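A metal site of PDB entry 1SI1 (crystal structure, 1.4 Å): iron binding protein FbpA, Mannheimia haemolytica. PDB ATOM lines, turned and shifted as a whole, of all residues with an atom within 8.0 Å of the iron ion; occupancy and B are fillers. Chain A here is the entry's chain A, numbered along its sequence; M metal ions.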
ATOM      1  N   TYR A   9      29.453 -19.866  -9.772  1.00  0.00           N
ATOM      2  CA  TYR A   9      28.438 -19.016  -9.157  1.00  0.00           C
ATOM      3  C   TYR A   9      28.052 -17.885 -10.108  1.00  0.00           C
ATOM      4  O   TYR A   9      26.924 -17.387 -10.094  1.00  0.00           O
ATOM      5  CB  TYR A   9      28.992 -18.449  -7.838  1.00  0.00           C
ATOM      6  CG  TYR A   9      28.275 -17.217  -7.370  1.00  0.00           C
ATOM      7  CD1 TYR A   9      27.149 -17.298  -6.554  1.00  0.00           C
ATOM      8  CD2 TYR A   9      28.722 -15.950  -7.745  1.00  0.00           C
ATOM      9  CE1 TYR A   9      26.497 -16.148  -6.137  1.00  0.00           C
ATOM     10  CE2 TYR A   9      28.079 -14.827  -7.357  1.00  0.00           C
ATOM     11  CZ  TYR A   9      26.969 -14.922  -6.547  1.00  0.00           C
ATOM     12  OH  TYR A   9      26.337 -13.750  -6.159  1.00  0.00           O
ATOM     13  N   ARG A  10      29.024 -17.420 -10.887  1.00  0.00           N
ATOM     14  CA  ARG A  10      28.824 -16.299 -11.786  1.00  0.00           C
ATOM     15  C   ARG A  10      28.108 -16.758 -13.053  1.00  0.00           C
ATOM     16  O   ARG A  10      28.336 -17.862 -13.540  1.00  0.00           O
ATOM     17  CB  ARG A  10      30.188 -15.701 -12.091  1.00  0.00           C
ATOM     18  CG  ARG A  10      30.229 -14.626 -13.141  1.00  0.00           C
ATOM     19  CD  ARG A  10      31.495 -13.794 -13.020  1.00  0.00           C
ATOM     20  NE  ARG A  10      31.348 -12.785 -11.985  1.00  0.00           N
ATOM     21  CZ  ARG A  10      32.274 -11.919 -11.626  1.00  0.00           C
ATOM     22  NH1 ARG A  10      31.971 -11.007 -10.728  1.00  0.00           N
ATOM     23  NH2 ARG A  10      33.491 -11.947 -12.140  1.00  0.00           N
ATOM     24  N   VAL A  58      32.503 -15.606  -6.426  1.00  0.00           N
ATOM     25  CA  VAL A  58      32.641 -14.179  -6.247  1.00  0.00           C
ATOM     26  C   VAL A  58      32.502 -13.887  -4.777  1.00  0.00           C
ATOM     27  O   VAL A  58      31.599 -14.414  -4.148  1.00  0.00           O
ATOM     28  CB  VAL A  58      31.535 -13.444  -7.042  1.00  0.00           C
ATOM     29  CG1 VAL A  58      31.573 -11.958  -6.759  1.00  0.00           C
ATOM     30  CG2 VAL A  58      31.656 -13.692  -8.549  1.00  0.00           C
ATOM     31  N   ASP A  59      33.381 -13.025  -4.288  1.00  0.00           N
ATOM     32  CA  ASP A  59      33.436 -12.533  -2.913  1.00  0.00           C
ATOM     33  C   ASP A  59      34.229 -13.476  -2.028  1.00  0.00           C
ATOM     34  O   ASP A  59      34.055 -14.690  -2.066  1.00  0.00           O
ATOM     35  CB  ASP A  59      32.037 -12.310  -2.334  1.00  0.00           C
ATOM     36  CG  ASP A  59      32.048 -11.427  -1.104  1.00  0.00           C
ATOM     37  OD1 ASP A  59      32.442 -11.891  -0.009  1.00  0.00           O
ATOM     38  OD2 ASP A  59      31.673 -10.258  -1.141  1.00  0.00           O
ATOM     39  N   ARG A  62      32.406 -16.256  -0.240  1.00  0.00           N
ATOM     40  CA  ARG A  62      32.067 -17.472  -0.962  1.00  0.00           C
ATOM     41  C   ARG A  62      33.285 -18.343  -1.186  1.00  0.00           C
ATOM     42  O   ARG A  62      33.186 -19.572  -1.198  1.00  0.00           O
ATOM     43  CB  ARG A  62      31.416 -17.142  -2.292  1.00  0.00           C
ATOM     44  CG  ARG A  62      30.100 -16.397  -2.147  1.00  0.00           C
ATOM     45  CD  ARG A  62      29.197 -16.500  -3.350  1.00  0.00           C
ATOM     46  NE  ARG A  62      27.971 -15.740  -3.142  1.00  0.00           N
ATOM     47  CZ  ARG A  62      27.851 -14.432  -3.265  1.00  0.00           C
ATOM     48  NH1 ARG A  62      26.670 -13.858  -3.038  1.00  0.00           N
ATOM     49  NH2 ARG A  62      28.889 -13.662  -3.615  1.00  0.00           N
ATOM     50  N   ARG A 101      36.889  -6.083  -7.101  1.00  0.00           N
ATOM     51  CA  ARG A 101      35.816  -5.124  -7.085  1.00  0.00           C
ATOM     52  C   ARG A 101      36.138  -4.156  -5.965  1.00  0.00           C
ATOM     53  O   ARG A 101      36.512  -4.559  -4.882  1.00  0.00           O
ATOM     54  CB  ARG A 101      34.468  -5.789  -6.882  1.00  0.00           C
ATOM     55  CG  ARG A 101      34.371  -6.758  -5.714  1.00  0.00           C
ATOM     56  CD  ARG A 101      34.389  -8.240  -6.087  1.00  0.00           C
ATOM     57  NE  ARG A 101      33.474  -8.545  -7.171  1.00  0.00           N
ATOM     58  CZ  ARG A 101      32.152  -8.785  -7.064  1.00  0.00           C
ATOM     59  NH1 ARG A 101      31.454  -9.011  -8.150  1.00  0.00           N
ATOM     60  NH2 ARG A 101      31.524  -8.791  -5.898  1.00  0.00           N
ATOM     61  N   ARG A 103      34.921  -1.371  -3.199  1.00  0.00           N
ATOM     62  CA  ARG A 103      33.770  -0.901  -2.460  1.00  0.00           C
ATOM     63  C   ARG A 103      33.946   0.602  -2.288  1.00  0.00           C
ATOM     64  O   ARG A 103      34.838   1.069  -1.597  1.00  0.00           O
ATOM     65  CB  ARG A 103      33.619  -1.623  -1.129  1.00  0.00           C
ATOM     66  CG  ARG A 103      32.252  -1.455  -0.485  1.00  0.00           C
ATOM     67  CD  ARG A 103      31.732  -2.708   0.176  1.00  0.00           C
ATOM     68  NE  ARG A 103      30.342  -2.584   0.604  1.00  0.00           N
ATOM     69  CZ  ARG A 103      29.300  -2.632  -0.220  1.00  0.00           C
ATOM     70  NH1 ARG A 103      28.064  -2.517   0.255  1.00  0.00           N
ATOM     71  NH2 ARG A 103      29.492  -2.807  -1.512  1.00  0.00           N
ATOM     72  N   ARG A 136      23.280  -0.917   2.511  1.00  0.00           N
ATOM     73  CA  ARG A 136      22.570  -2.184   2.624  1.00  0.00           C
ATOM     74  C   ARG A 136      22.932  -2.857   3.954  1.00  0.00           C
ATOM     75  O   ARG A 136      23.810  -2.396   4.687  1.00  0.00           O
ATOM     76  CB  ARG A 136      22.908  -3.101   1.448  1.00  0.00           C
ATOM     77  CG  ARG A 136      24.288  -3.733   1.540  1.00  0.00           C
ATOM     78  CD  ARG A 136      24.637  -4.544   0.348  1.00  0.00           C
ATOM     79  NE  ARG A 136      23.692  -5.639   0.154  1.00  0.00           N
ATOM     80  CZ  ARG A 136      23.621  -6.352  -0.952  1.00  0.00           C
ATOM     81  NH1 ARG A 136      24.420  -6.094  -1.976  1.00  0.00           N
ATOM     82  NH2 ARG A 136      22.729  -7.328  -1.030  1.00  0.00           N
ATOM     83  N   ASN A 140      25.559  -8.138   5.050  1.00  0.00           N
ATOM     84  CA  ASN A 140      25.903  -8.499   3.689  1.00  0.00           C
ATOM     85  C   ASN A 140      27.403  -8.587   3.545  1.00  0.00           C
ATOM     86  O   ASN A 140      28.137  -7.787   4.114  1.00  0.00           O
ATOM     87  CB  ASN A 140      25.362  -7.496   2.688  1.00  0.00           C
ATOM     88  CG  ASN A 140      25.748  -7.859   1.279  1.00  0.00           C
ATOM     89  OD1 ASN A 140      25.136  -8.726   0.664  1.00  0.00           O
ATOM     90  ND2 ASN A 140      26.796  -7.243   0.796  1.00  0.00           N
ATOM     91  N   SER A 141      27.861  -9.580   2.780  1.00  0.00           N
ATOM     92  CA  SER A 141      29.281  -9.891   2.697  1.00  0.00           C
ATOM     93  C   SER A 141      30.105  -8.733   2.196  1.00  0.00           C
ATOM     94  O   SER A 141      31.251  -8.584   2.602  1.00  0.00           O
ATOM     95  CB  SER A 141      29.522 -11.114   1.803  1.00  0.00           C
ATOM     96  OG  SER A 141      29.255 -10.822   0.447  1.00  0.00           O
ATOM     97  N   TYR A 142      29.555  -7.910   1.307  1.00  0.00           N
ATOM     98  CA  TYR A 142      30.317  -6.772   0.831  1.00  0.00           C
ATOM     99  C   TYR A 142      30.687  -5.855   1.984  1.00  0.00           C
ATOM    100  O   TYR A 142      31.807  -5.332   2.050  1.00  0.00           O
ATOM    101  CB  TYR A 142      29.546  -5.962  -0.204  1.00  0.00           C
ATOM    102  CG  TYR A 142      29.039  -6.704  -1.407  1.00  0.00           C
ATOM    103  CD1 TYR A 142      29.636  -7.874  -1.863  1.00  0.00           C
ATOM    104  CD2 TYR A 142      27.975  -6.190  -2.108  1.00  0.00           C
ATOM    105  CE1 TYR A 142      29.135  -8.528  -2.982  1.00  0.00           C
ATOM    106  CE2 TYR A 142      27.495  -6.825  -3.247  1.00  0.00           C
ATOM    107  CZ  TYR A 142      28.072  -7.989  -3.656  1.00  0.00           C
ATOM    108  OH  TYR A 142      27.541  -8.580  -4.787  1.00  0.00           O
ATOM    109  N   ASP A 178      23.142  -2.928  -3.294  1.00  0.00           N
ATOM    110  CA  ASP A 178      23.970  -1.748  -3.551  1.00  0.00           C
ATOM    111  C   ASP A 178      23.316  -0.791  -4.536  1.00  0.00           C
ATOM    112  O   ASP A 178      23.342   0.410  -4.344  1.00  0.00           O
ATOM    113  CB  ASP A 178      25.331  -2.155  -4.108  1.00  0.00           C
ATOM    114  CG  ASP A 178      26.299  -2.618  -3.067  1.00  0.00           C
ATOM    115  OD1 ASP A 178      25.962  -2.628  -1.862  1.00  0.00           O
ATOM    116  OD2 ASP A 178      27.452  -2.966  -3.380  1.00  0.00           O
ATOM    117  N   ARG A 179      22.719  -1.325  -5.600  1.00  0.00           N
ATOM    118  CA  ARG A 179      22.072  -0.476  -6.583  1.00  0.00           C
ATOM    119  C   ARG A 179      20.916   0.306  -5.963  1.00  0.00           C
ATOM    120  O   ARG A 179      20.703   1.451  -6.301  1.00  0.00           O
ATOM    121  CB  ARG A 179      21.542  -1.317  -7.734  1.00  0.00           C
ATOM    122  CG  ARG A 179      22.602  -1.967  -8.608  1.00  0.00           C
ATOM    123  CD  ARG A 179      22.068  -2.967  -9.601  1.00  0.00           C
ATOM    124  NE  ARG A 179      21.482  -4.122  -8.916  1.00  0.00           N
ATOM    125  CZ  ARG A 179      20.549  -4.921  -9.434  1.00  0.00           C
ATOM    126  NH1 ARG A 179      20.097  -4.759 -10.679  1.00  0.00           N
ATOM    127  NH2 ARG A 179      20.079  -5.927  -8.708  1.00  0.00           N
ATOM    128  N   ASN A 196      29.481  -1.374  -4.464  1.00  0.00           N
ATOM    129  CA  ASN A 196      30.586  -1.835  -5.288  1.00  0.00           C
ATOM    130  C   ASN A 196      30.678  -1.040  -6.582  1.00  0.00           C
ATOM    131  O   ASN A 196      29.668  -0.644  -7.144  1.00  0.00           O
ATOM    132  CB  ASN A 196      30.462  -3.315  -5.587  1.00  0.00           C
ATOM    133  CG  ASN A 196      30.763  -4.177  -4.389  1.00  0.00           C
ATOM    134  OD1 ASN A 196      31.437  -3.757  -3.438  1.00  0.00           O
ATOM    135  ND2 ASN A 196      30.302  -5.406  -4.429  1.00  0.00           N
ATOM    136  N   TYR A 198      31.538  -1.900  -9.635  1.00  0.00           N
ATOM    137  CA  TYR A 198      31.056  -2.490 -10.887  1.00  0.00           C
ATOM    138  C   TYR A 198      29.581  -2.197 -11.102  1.00  0.00           C
ATOM    139  O   TYR A 198      29.119  -2.184 -12.227  1.00  0.00           O
ATOM    140  CB  TYR A 198      31.320  -3.997 -10.960  1.00  0.00           C
ATOM    141  CG  TYR A 198      30.712  -4.783  -9.836  1.00  0.00           C
ATOM    142  CD1 TYR A 198      31.457  -5.106  -8.716  1.00  0.00           C
ATOM    143  CD2 TYR A 198      29.383  -5.164  -9.856  1.00  0.00           C
ATOM    144  CE1 TYR A 198      30.922  -5.794  -7.703  1.00  0.00           C
ATOM    145  CE2 TYR A 198      28.825  -5.868  -8.833  1.00  0.00           C
ATOM    146  CZ  TYR A 198      29.588  -6.179  -7.745  1.00  0.00           C
ATOM    147  OH  TYR A 198      29.047  -6.858  -6.666  1.00  0.00           O
ATOM    148  N   TYR A 199      28.834  -1.919 -10.024  1.00  0.00           N
ATOM    149  CA  TYR A 199      27.416  -1.612 -10.182  1.00  0.00           C
ATOM    150  C   TYR A 199      27.185  -0.327 -10.961  1.00  0.00           C
ATOM    151  O   TYR A 199      26.163  -0.160 -11.578  1.00  0.00           O
ATOM    152  CB  TYR A 199      26.708  -1.510  -8.821  1.00  0.00           C
ATOM    153  CG  TYR A 199      26.485  -2.849  -8.195  1.00  0.00           C
ATOM    154  CD1 TYR A 199      27.047  -3.153  -6.970  1.00  0.00           C
ATOM    155  CD2 TYR A 199      25.730  -3.821  -8.824  1.00  0.00           C
ATOM    156  CE1 TYR A 199      26.867  -4.369  -6.382  1.00  0.00           C
ATOM    157  CE2 TYR A 199      25.535  -5.053  -8.238  1.00  0.00           C
ATOM    158  CZ  TYR A 199      26.114  -5.318  -7.027  1.00  0.00           C
ATOM    159  OH  TYR A 199      25.955  -6.556  -6.459  1.00  0.00           O
ATOM    160  N   LYS A 202      27.044  -1.566 -14.375  1.00  0.00           N
ATOM    161  CA  LYS A 202      25.841  -2.365 -14.581  1.00  0.00           C
ATOM    162  C   LYS A 202      24.604  -1.490 -14.707  1.00  0.00           C
ATOM    163  O   LYS A 202      23.733  -1.744 -15.536  1.00  0.00           O
ATOM    164  CB  LYS A 202      25.658  -3.368 -13.440  1.00  0.00           C
ATOM    165  CG  LYS A 202      26.855  -4.286 -13.256  1.00  0.00           C
ATOM    166  CD  LYS A 202      26.486  -5.725 -13.123  1.00  0.00           C
ATOM    167  CE  LYS A 202      27.730  -6.598 -13.018  1.00  0.00           C
ATOM    168  NZ  LYS A 202      27.760  -7.633 -14.083  1.00  0.00           N
ATOM    169  N   GLU A 268      34.861  -4.991 -13.617  1.00  0.00           N
ATOM    170  CA  GLU A 268      35.766  -5.167 -12.495  1.00  0.00           C
ATOM    171  C   GLU A 268      37.178  -4.776 -12.891  1.00  0.00           C
ATOM    172  O   GLU A 268      37.409  -4.322 -14.000  1.00  0.00           O
ATOM    173  CB  GLU A 268      35.703  -6.621 -12.037  1.00  0.00           C
ATOM    174  CG  GLU A 268      34.395  -6.952 -11.360  1.00  0.00           C
ATOM    175  CD  GLU A 268      34.217  -8.408 -11.041  1.00  0.00           C
ATOM    176  OE1 GLU A 268      33.432  -8.691 -10.119  1.00  0.00           O
ATOM    177  OE2 GLU A 268      34.795  -9.271 -11.729  1.00  0.00           O
HETATM  178 FE    FE M   1      27.367  -7.877  -6.658  1.00  0.00          FE
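Of the 18 residues printed, 3 come within 4 Å of the iron ion.
The nearest printed residue that does not touch the iron ion is Arg 101 (4.3 Å).
The iron ion is bound by OH of Tyr 199, OH of Tyr 198 and OH of Tyr 142.
The iron ion has three donor atoms within binding distance.
The side-chain hydroxyl (OH) of Tyr 198 sits close to the guanidinium group (NH2) of Arg 101 (3.2 Å).
OH of Tyr 198 sits close to ND2 of Asn 196.
The backbone NH (N) of Tyr 142 sits close to the side-chain amide nitrogen (ND2) of Asn 140.
The backbone carbonyl oxygen (O) of Tyr 142 lies close to the guanidinium group (NE) of Arg 103 (3.4 Å).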
